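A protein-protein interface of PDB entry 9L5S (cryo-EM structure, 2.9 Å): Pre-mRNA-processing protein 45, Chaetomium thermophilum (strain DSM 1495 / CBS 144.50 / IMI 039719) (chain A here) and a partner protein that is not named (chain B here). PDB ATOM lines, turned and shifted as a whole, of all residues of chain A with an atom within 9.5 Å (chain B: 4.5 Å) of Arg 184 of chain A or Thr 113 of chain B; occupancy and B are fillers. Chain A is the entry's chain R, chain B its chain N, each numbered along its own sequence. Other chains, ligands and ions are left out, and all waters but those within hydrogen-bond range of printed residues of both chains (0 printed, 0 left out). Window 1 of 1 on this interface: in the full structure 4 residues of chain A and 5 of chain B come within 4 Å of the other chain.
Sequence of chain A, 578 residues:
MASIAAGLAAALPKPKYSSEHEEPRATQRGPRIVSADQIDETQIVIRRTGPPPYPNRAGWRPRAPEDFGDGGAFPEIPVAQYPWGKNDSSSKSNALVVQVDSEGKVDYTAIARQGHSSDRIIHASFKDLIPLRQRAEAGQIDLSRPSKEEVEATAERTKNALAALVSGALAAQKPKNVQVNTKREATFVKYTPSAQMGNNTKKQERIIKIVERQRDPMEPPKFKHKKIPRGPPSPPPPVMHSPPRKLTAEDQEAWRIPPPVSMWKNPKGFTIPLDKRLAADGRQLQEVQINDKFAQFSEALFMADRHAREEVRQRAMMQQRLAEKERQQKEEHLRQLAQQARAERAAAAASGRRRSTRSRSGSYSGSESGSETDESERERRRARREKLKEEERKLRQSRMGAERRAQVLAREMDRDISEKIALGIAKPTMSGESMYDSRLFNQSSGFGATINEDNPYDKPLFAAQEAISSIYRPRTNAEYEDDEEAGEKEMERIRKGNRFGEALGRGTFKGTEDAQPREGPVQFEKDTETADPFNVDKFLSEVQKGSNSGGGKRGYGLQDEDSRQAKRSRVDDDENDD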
ATOM      1  N   VAL A 180     -15.914  30.044  16.212  1.00  0.00           N
ATOM      2  CA  VAL A 180     -14.471  30.113  16.017  1.00  0.00           C
ATOM      3  C   VAL A 180     -13.937  31.408  16.606  1.00  0.00           C
ATOM      4  O   VAL A 180     -14.659  32.398  16.753  1.00  0.00           O
ATOM      5  CB  VAL A 180     -14.060  29.997  14.534  1.00  0.00           C
ATOM      6  CG1 VAL A 180     -14.194  28.563  14.072  1.00  0.00           C
ATOM      7  CG2 VAL A 180     -14.879  30.940  13.672  1.00  0.00           C
ATOM      8  N   ASN A 181     -12.650  31.385  16.946  1.00  0.00           N
ATOM      9  CA  ASN A 181     -11.975  32.533  17.546  1.00  0.00           C
ATOM     10  C   ASN A 181     -10.541  32.516  17.035  1.00  0.00           C
ATOM     11  O   ASN A 181      -9.747  31.666  17.451  1.00  0.00           O
ATOM     12  CB  ASN A 181     -12.028  32.464  19.072  1.00  0.00           C
ATOM     13  CG  ASN A 181     -11.565  33.750  19.740  1.00  0.00           C
ATOM     14  OD1 ASN A 181     -11.156  34.704  19.078  1.00  0.00           O
ATOM     15  ND2 ASN A 181     -11.634  33.777  21.067  1.00  0.00           N
ATOM     16  N   THR A 182     -10.216  33.437  16.134  1.00  0.00           N
ATOM     17  CA  THR A 182      -8.888  33.509  15.544  1.00  0.00           C
ATOM     18  C   THR A 182      -7.945  34.416  16.325  1.00  0.00           C
ATOM     19  O   THR A 182      -6.825  34.664  15.869  1.00  0.00           O
ATOM     20  CB  THR A 182      -8.979  33.979  14.089  1.00  0.00           C
ATOM     21  OG1 THR A 182      -9.598  35.270  14.039  1.00  0.00           O
ATOM     22  CG2 THR A 182      -9.796  32.997  13.266  1.00  0.00           C
ATOM     23  N   LYS A 183      -8.372  34.910  17.484  1.00  0.00           N
ATOM     24  CA  LYS A 183      -7.498  35.647  18.398  1.00  0.00           C
ATOM     25  C   LYS A 183      -6.823  34.695  19.381  1.00  0.00           C
ATOM     26  O   LYS A 183      -6.920  34.838  20.599  1.00  0.00           O
ATOM     27  CB  LYS A 183      -8.294  36.722  19.128  1.00  0.00           C
ATOM     28  CG  LYS A 183      -9.201  37.541  18.225  1.00  0.00           C
ATOM     29  CD  LYS A 183      -9.952  38.605  19.008  1.00  0.00           C
ATOM     30  CE  LYS A 183     -10.997  39.291  18.141  1.00  0.00           C
ATOM     31  NZ  LYS A 183     -12.189  38.429  17.915  1.00  0.00           N
ATOM     32  N   ARG A 184      -6.129  33.700  18.830  1.00  0.00           N
ATOM     33  CA  ARG A 184      -5.563  32.596  19.603  1.00  0.00           C
ATOM     34  C   ARG A 184      -4.231  33.039  20.204  1.00  0.00           C
ATOM     35  O   ARG A 184      -3.147  32.732  19.702  1.00  0.00           O
ATOM     36  CB  ARG A 184      -5.393  31.372  18.715  1.00  0.00           C
ATOM     37  CG  ARG A 184      -6.657  30.559  18.514  1.00  0.00           C
ATOM     38  CD  ARG A 184      -6.373  29.374  17.617  1.00  0.00           C
ATOM     39  NE  ARG A 184      -5.411  29.715  16.576  1.00  0.00           N
ATOM     40  CZ  ARG A 184      -4.347  28.986  16.267  1.00  0.00           C
ATOM     41  NH1 ARG A 184      -4.069  27.863  16.906  1.00  0.00           N
ATOM     42  NH2 ARG A 184      -3.544  29.395  15.288  1.00  0.00           N
ATOM     43  N   GLU A 185      -4.321  33.776  21.308  1.00  0.00           N
ATOM     44  CA  GLU A 185      -3.126  34.246  21.994  1.00  0.00           C
ATOM     45  C   GLU A 185      -2.520  33.119  22.820  1.00  0.00           C
ATOM     46  O   GLU A 185      -3.230  32.427  23.558  1.00  0.00           O
ATOM     47  CB  GLU A 185      -3.452  35.445  22.882  1.00  0.00           C
ATOM     48  CG  GLU A 185      -2.227  36.214  23.346  1.00  0.00           C
ATOM     49  CD  GLU A 185      -2.573  37.574  23.914  1.00  0.00           C
ATOM     50  OE1 GLU A 185      -3.768  37.939  23.903  1.00  0.00           O
ATOM     51  OE2 GLU A 185      -1.650  38.281  24.368  1.00  0.00           O
ATOM     52  N   ALA A 186      -1.211  32.938  22.695  1.00  0.00           N
ATOM     53  CA  ALA A 186      -0.516  31.846  23.354  1.00  0.00           C
ATOM     54  C   ALA A 186      -0.365  32.111  24.849  1.00  0.00           C
ATOM     55  O   ALA A 186      -0.369  33.254  25.313  1.00  0.00           O
ATOM     56  CB  ALA A 186       0.858  31.628  22.725  1.00  0.00           C
ATOM     57  N   THR A 187      -0.231  31.024  25.603  1.00  0.00           N
ATOM     58  CA  THR A 187       0.019  31.072  27.037  1.00  0.00           C
ATOM     59  C   THR A 187       1.347  30.382  27.317  1.00  0.00           C
ATOM     60  O   THR A 187       1.567  29.254  26.869  1.00  0.00           O
ATOM     61  CB  THR A 187      -1.115  30.398  27.817  1.00  0.00           C
ATOM     62  OG1 THR A 187      -2.340  31.103  27.587  1.00  0.00           O
ATOM     63  CG2 THR A 187      -0.823  30.396  29.308  1.00  0.00           C
ATOM     64  N   PHE A 188       2.228  31.049  28.051  1.00  0.00           N
ATOM     65  CA  PHE A 188       3.553  30.512  28.324  1.00  0.00           C
ATOM     66  C   PHE A 188       3.606  29.979  29.748  1.00  0.00           C
ATOM     67  O   PHE A 188       3.123  30.625  30.682  1.00  0.00           O
ATOM     68  CB  PHE A 188       4.629  31.574  28.108  1.00  0.00           C
ATOM     69  CG  PHE A 188       4.739  32.036  26.683  1.00  0.00           C
ATOM     70  CD1 PHE A 188       5.493  31.325  25.765  1.00  0.00           C
ATOM     71  CD2 PHE A 188       4.087  33.184  26.263  1.00  0.00           C
ATOM     72  CE1 PHE A 188       5.594  31.751  24.455  1.00  0.00           C
ATOM     73  CE2 PHE A 188       4.186  33.614  24.956  1.00  0.00           C
ATOM     74  CZ  PHE A 188       4.940  32.897  24.051  1.00  0.00           C
ATOM     75  N   LYS A 209       4.902  26.701  25.268  1.00  0.00           N
ATOM     76  CA  LYS A 209       3.910  27.533  24.600  1.00  0.00           C
ATOM     77  C   LYS A 209       2.652  26.705  24.370  1.00  0.00           C
ATOM     78  O   LYS A 209       2.698  25.679  23.685  1.00  0.00           O
ATOM     79  CB  LYS A 209       4.467  28.051  23.275  1.00  0.00           C
ATOM     80  CG  LYS A 209       3.629  29.107  22.582  1.00  0.00           C
ATOM     81  CD  LYS A 209       4.327  29.590  21.320  1.00  0.00           C
ATOM     82  CE  LYS A 209       3.362  30.280  20.372  1.00  0.00           C
ATOM     83  NZ  LYS A 209       4.069  30.932  19.236  1.00  0.00           N
ATOM     84  N   ILE A 210       1.534  27.146  24.937  1.00  0.00           N
ATOM     85  CA  ILE A 210       0.261  26.448  24.832  1.00  0.00           C
ATOM     86  C   ILE A 210      -0.685  27.329  24.031  1.00  0.00           C
ATOM     87  O   ILE A 210      -0.991  28.456  24.441  1.00  0.00           O
ATOM     88  CB  ILE A 210      -0.327  26.116  26.212  1.00  0.00           C
ATOM     89  CG1 ILE A 210       0.652  25.248  27.008  1.00  0.00           C
ATOM     90  CG2 ILE A 210      -1.670  25.423  26.064  1.00  0.00           C
ATOM     91  CD1 ILE A 210       0.121  24.789  28.346  1.00  0.00           C
ATOM     92  N   VAL A 211      -1.137  26.817  22.890  1.00  0.00           N
ATOM     93  CA  VAL A 211      -2.015  27.533  21.977  1.00  0.00           C
ATOM     94  C   VAL A 211      -3.272  26.694  21.790  1.00  0.00           C
ATOM     95  O   VAL A 211      -3.205  25.465  21.714  1.00  0.00           O
ATOM     96  CB  VAL A 211      -1.318  27.805  20.620  1.00  0.00           C
ATOM     97  CG1 VAL A 211      -2.210  28.605  19.684  1.00  0.00           C
ATOM     98  CG2 VAL A 211       0.009  28.512  20.825  1.00  0.00           C
ATOM     99  N   GLU A 212      -4.424  27.359  21.753  1.00  0.00           N
ATOM    100  CA  GLU A 212      -5.661  26.676  21.402  1.00  0.00           C
ATOM    101  C   GLU A 212      -5.585  26.173  19.963  1.00  0.00           C
ATOM    102  O   GLU A 212      -5.034  26.833  19.080  1.00  0.00           O
ATOM    103  CB  GLU A 212      -6.855  27.616  21.581  1.00  0.00           C
ATOM    104  CG  GLU A 212      -8.210  26.980  21.319  1.00  0.00           C
ATOM    105  CD  GLU A 212      -9.361  27.938  21.558  1.00  0.00           C
ATOM    106  OE1 GLU A 212      -9.101  29.108  21.907  1.00  0.00           O
ATOM    107  OE2 GLU A 212     -10.527  27.519  21.399  1.00  0.00           O
ATOM    108  N   ARG A 213      -6.111  24.972  19.738  1.00  0.00           N
ATOM    109  CA  ARG A 213      -6.065  24.372  18.413  1.00  0.00           C
ATOM    110  C   ARG A 213      -7.125  24.987  17.506  1.00  0.00           C
ATOM    111  O   ARG A 213      -8.247  25.265  17.937  1.00  0.00           O
ATOM    112  CB  ARG A 213      -6.273  22.859  18.495  1.00  0.00           C
ATOM    113  CG  ARG A 213      -5.982  22.141  17.188  1.00  0.00           C
ATOM    114  CD  ARG A 213      -6.318  20.669  17.254  1.00  0.00           C
ATOM    115  NE  ARG A 213      -7.762  20.463  17.253  1.00  0.00           N
ATOM    116  CZ  ARG A 213      -8.509  20.374  16.161  1.00  0.00           C
ATOM    117  NH1 ARG A 213      -7.987  20.501  14.953  1.00  0.00           N
ATOM    118  NH2 ARG A 213      -9.816  20.163  16.286  1.00  0.00           N
ATOM    119  N   GLN A 214      -6.754  25.207  16.246  1.00  0.00           N
ATOM    120  CA  GLN A 214      -7.703  25.651  15.231  1.00  0.00           C
ATOM    121  C   GLN A 214      -8.745  24.567  14.984  1.00  0.00           C
ATOM    122  O   GLN A 214      -8.406  23.449  14.587  1.00  0.00           O
ATOM    123  CB  GLN A 214      -6.967  25.985  13.938  1.00  0.00           C
ATOM    124  CG  GLN A 214      -6.332  27.356  13.924  1.00  0.00           C
ATOM    125  CD  GLN A 214      -5.224  27.473  12.898  1.00  0.00           C
ATOM    126  OE1 GLN A 214      -4.590  26.483  12.537  1.00  0.00           O
ATOM    127  NE2 GLN A 214      -4.984  28.689  12.423  1.00  0.00           N
ATOM    128  N   ARG A 215     -10.011  24.898  15.216  1.00  0.00           N
ATOM    129  CA  ARG A 215     -11.109  23.960  15.034  1.00  0.00           C
ATOM    130  C   ARG A 215     -11.871  24.286  13.759  1.00  0.00           C
ATOM    131  O   ARG A 215     -12.025  25.456  13.397  1.00  0.00           O
ATOM    132  CB  ARG A 215     -12.064  23.988  16.229  1.00  0.00           C
ATOM    133  CG  ARG A 215     -11.483  23.404  17.500  1.00  0.00           C
ATOM    134  CD  ARG A 215     -12.531  23.315  18.597  1.00  0.00           C
ATOM    135  NE  ARG A 215     -13.370  24.506  18.650  1.00  0.00           N
ATOM    136  CZ  ARG A 215     -13.048  25.620  19.294  1.00  0.00           C
ATOM    137  NH1 ARG A 215     -11.899  25.738  19.938  1.00  0.00           N
ATOM    138  NH2 ARG A 215     -13.899  26.642  19.287  1.00  0.00           N
ATOM    139  N   GLN B 109       1.262  32.242   4.875  1.00  0.00           N
ATOM    140  CA  GLN B 109       0.099  32.686   5.637  1.00  0.00           C
ATOM    141  C   GLN B 109       0.320  32.280   7.087  1.00  0.00           C
ATOM    142  O   GLN B 109      -0.033  31.180   7.511  1.00  0.00           O
ATOM    143  CB  GLN B 109      -1.181  32.086   5.071  1.00  0.00           C
ATOM    144  CG  GLN B 109      -2.447  32.659   5.675  1.00  0.00           C
ATOM    145  CD  GLN B 109      -2.417  34.170   5.752  1.00  0.00           C
ATOM    146  OE1 GLN B 109      -2.395  34.745   6.837  1.00  0.00           O
ATOM    147  NE2 GLN B 109      -2.412  34.820   4.598  1.00  0.00           N
ATOM    148  N   THR B 110       0.919  33.188   7.859  1.00  0.00           N
ATOM    149  CA  THR B 110       1.276  32.882   9.237  1.00  0.00           C
ATOM    150  C   THR B 110       0.073  32.866  10.166  1.00  0.00           C
ATOM    151  O   THR B 110       0.129  32.224  11.217  1.00  0.00           O
ATOM    152  CB  THR B 110       2.303  33.888   9.751  1.00  0.00           C
ATOM    153  OG1 THR B 110       1.854  35.217   9.462  1.00  0.00           O
ATOM    154  CG2 THR B 110       3.643  33.656   9.094  1.00  0.00           C
ATOM    155  N   LYS B 111      -1.015  33.538   9.804  1.00  0.00           N
ATOM    156  CA  LYS B 111      -2.205  33.562  10.643  1.00  0.00           C
ATOM    157  C   LYS B 111      -2.962  32.242  10.643  1.00  0.00           C
ATOM    158  O   LYS B 111      -3.887  32.080  11.445  1.00  0.00           O
ATOM    159  CB  LYS B 111      -3.142  34.687  10.200  1.00  0.00           C
ATOM    160  CG  LYS B 111      -2.649  36.083  10.542  1.00  0.00           C
ATOM    161  CD  LYS B 111      -3.614  37.146  10.040  1.00  0.00           C
ATOM    162  CE  LYS B 111      -3.493  37.334   8.538  1.00  0.00           C
ATOM    163  NZ  LYS B 111      -4.349  38.440   8.032  1.00  0.00           N
ATOM    164  N   GLU B 112      -2.598  31.299   9.774  1.00  0.00           N
ATOM    165  CA  GLU B 112      -3.362  30.073   9.587  1.00  0.00           C
ATOM    166  C   GLU B 112      -2.558  28.817   9.903  1.00  0.00           C
ATOM    167  O   GLU B 112      -2.908  27.729   9.436  1.00  0.00           O
ATOM    168  CB  GLU B 112      -3.909  30.020   8.164  1.00  0.00           C
ATOM    169  CG  GLU B 112      -5.122  30.902   7.981  1.00  0.00           C
ATOM    170  CD  GLU B 112      -5.530  31.051   6.539  1.00  0.00           C
ATOM    171  OE1 GLU B 112      -5.327  30.100   5.757  1.00  0.00           O
ATOM    172  OE2 GLU B 112      -6.063  32.120   6.196  1.00  0.00           O
ATOM    173  N   THR B 113      -1.489  28.941  10.680  1.00  0.00           N
ATOM    174  CA  THR B 113      -0.772  27.794  11.213  1.00  0.00           C
ATOM    175  C   THR B 113      -1.052  27.673  12.705  1.00  0.00           C
ATOM    176  O   THR B 113      -1.640  28.566  13.321  1.00  0.00           O
ATOM    177  CB  THR B 113       0.734  27.908  10.960  1.00  0.00           C
ATOM    178  OG1 THR B 113       1.172  29.235  11.266  1.00  0.00           O
ATOM    179  CG2 THR B 113       1.053  27.597   9.506  1.00  0.00           C
ATOM    180  N   ASN B 114      -0.639  26.537  13.276  1.00  0.00           N
ATOM    181  CA  ASN B 114      -0.922  26.256  14.681  1.00  0.00           C
ATOM    182  C   ASN B 114      -0.197  27.227  15.604  1.00  0.00           C
ATOM    183  O   ASN B 114      -0.779  27.737  16.568  1.00  0.00           O
ATOM    184  CB  ASN B 114      -0.537  24.815  15.019  1.00  0.00           C
ATOM    185  CG  ASN B 114      -1.476  23.797  14.402  1.00  0.00           C
ATOM    186  OD1 ASN B 114      -2.681  24.020  14.315  1.00  0.00           O
ATOM    187  ND2 ASN B 114      -0.926  22.663  13.982  1.00  0.00           N
ATOM    188  N   PHE B 115       1.075  27.501  15.322  1.00  0.00           N
ATOM    189  CA  PHE B 115       1.914  28.318  16.189  1.00  0.00           C
ATOM    190  C   PHE B 115       2.391  29.587  15.494  1.00  0.00           C
ATOM    191  O   PHE B 115       3.442  30.131  15.843  1.00  0.00           O
ATOM    192  CB  PHE B 115       3.094  27.497  16.699  1.00  0.00           C
ATOM    193  CG  PHE B 115       2.680  26.258  17.431  1.00  0.00           C
ATOM    194  CD1 PHE B 115       2.133  26.342  18.700  1.00  0.00           C
ATOM    195  CD2 PHE B 115       2.812  25.012  16.842  1.00  0.00           C
ATOM    196  CE1 PHE B 115       1.738  25.205  19.371  1.00  0.00           C
ATOM    197  CE2 PHE B 115       2.420  23.872  17.510  1.00  0.00           C
ATOM    198  CZ  PHE B 115       1.881  23.969  18.775  1.00  0.00           C
ATOM    199  N   ASN B 116       1.617  30.053  14.509  1.00  0.00           N
ATOM    200  CA  ASN B 116       1.872  31.294  13.772  1.00  0.00           C
ATOM    201  C   ASN B 116       3.235  31.275  13.085  1.00  0.00           C
ATOM    202  O   ASN B 116       3.973  32.261  13.082  1.00  0.00           O
ATOM    203  CB  ASN B 116       1.722  32.515  14.677  1.00  0.00           C
ATOM    204  CG  ASN B 116       0.305  32.695  15.175  1.00  0.00           C
ATOM    205  OD1 ASN B 116       0.072  32.876  16.369  1.00  0.00           O
ATOM    206  ND2 ASN B 116      -0.653  32.651  14.259  1.00  0.00           N
ATOM    207  N   SER B 117       3.567  30.134  12.497  1.00  0.00           N
ATOM    208  CA  SER B 117       4.794  29.960  11.741  1.00  0.00           C
ATOM    209  C   SER B 117       4.515  30.058  10.246  1.00  0.00           C
ATOM    210  O   SER B 117       3.367  30.057   9.797  1.00  0.00           O
ATOM    211  CB  SER B 117       5.438  28.611  12.076  1.00  0.00           C
ATOM    212  OG  SER B 117       5.432  28.371  13.472  1.00  0.00           O
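Arg 184 of chain A touches two residues of chain B.
Thr 113 of chain B touches just these residues of chain A: Arg 184 and Gln 214.
Asn 116 of chain B touches none of the printed residues of chain A.
Of the printed residues of chain B, Val 211 of chain A touches Asn 114 (3.5 Å) and Phe 115 (3.7 Å).
Of the printed residues of chain B, Gln 214 of chain A touches Lys 111, Glu 112, Thr 113 and Asn 114.
Of the printed residues of chain A, Phe 115 of chain B touches Lys 209 and Val 211.
Of the printed residues of chain B, Lys 209 of chain A touches Phe 115 (3.5 Å).
Of the printed residues of chain A, Glu 112 of chain B touches Gln 214.
Thr 110 of chain B touches none of the printed residues of chain A.
Phe 188 of chain A touches none of the printed residues of chain B.
The nearest residue of chain A that does not touch Thr 113 of chain B is Val 211 of chain A (6.4 Å).
The nearest printed residue of chain B that does not touch Val 211 of chain A is Asn 116 of chain B (5.9 Å).
OG1 of Thr 113 of chain B is in hydrogen-bond range of O of Thr 110 of chain B, 3.2 Å away.
The backbone NH (N) of Lys 111 of chain B sits close to the side-chain amide oxygen (OE1) of Gln 109 of chain B (3.5 Å).
The side-chain amide nitrogen (NE2) of Gln 214 of chain A lies close to the guanidinium group (NH2) of Arg 184 of chain A (3.3 Å).
The side-chain hydroxyl (OG1) of Thr 113 of chain B lies within hydrogen-bond range of the backbone carbonyl oxygen (O) of Ser 117 of chain B.
The side-chain hydroxyl (OG1) of Thr 113 of chain B sits close to the backbone NH (N) of Asn 116 of chain B, at 3.4 Å.
O of Glu 212 of chain A is in hydrogen-bond range of NH1 of Arg 184 of chain A.
Of the 9 printed residues of chain B, 5 touch a printed residue of chain A.
Printed residues of chain A that touch a printed residue of chain B: Arg 184, Lys 209, Val 211 and Gln 214.
Among the printed residues, 9 pairs touch across the chains.
Among the printed residues, no Asp or Glu carboxylate lies within 4 Å of a Lys or Arg side-chain nitrogen of the other chain.
O of Asn 114 of chain B is in hydrogen-bond range of NH1 of Arg 184 of chain A (3.3 Å).
NE2 of Gln 214 of chain A sits at hydrogen-bond distance from O of Thr 113 of chain B, 3.5 Å away.
NH2 of Arg 184 of chain A lies within hydrogen-bond range of O of Thr 113 of chain B (2.9 Å).
Among the printed residues, merely in contact across the chains: Gln 214 of chain A with Glu 112 of chain B, Val 211 of chain A with Asn 114 of chain B, Lys 209 of chain A with Phe 115 of chain B, Gln 214 of chain A with Asn 114 of chain B, Gln 214 of chain A with Lys 111 of chain B and Val 211 of chain A with Phe 115 of chain B.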
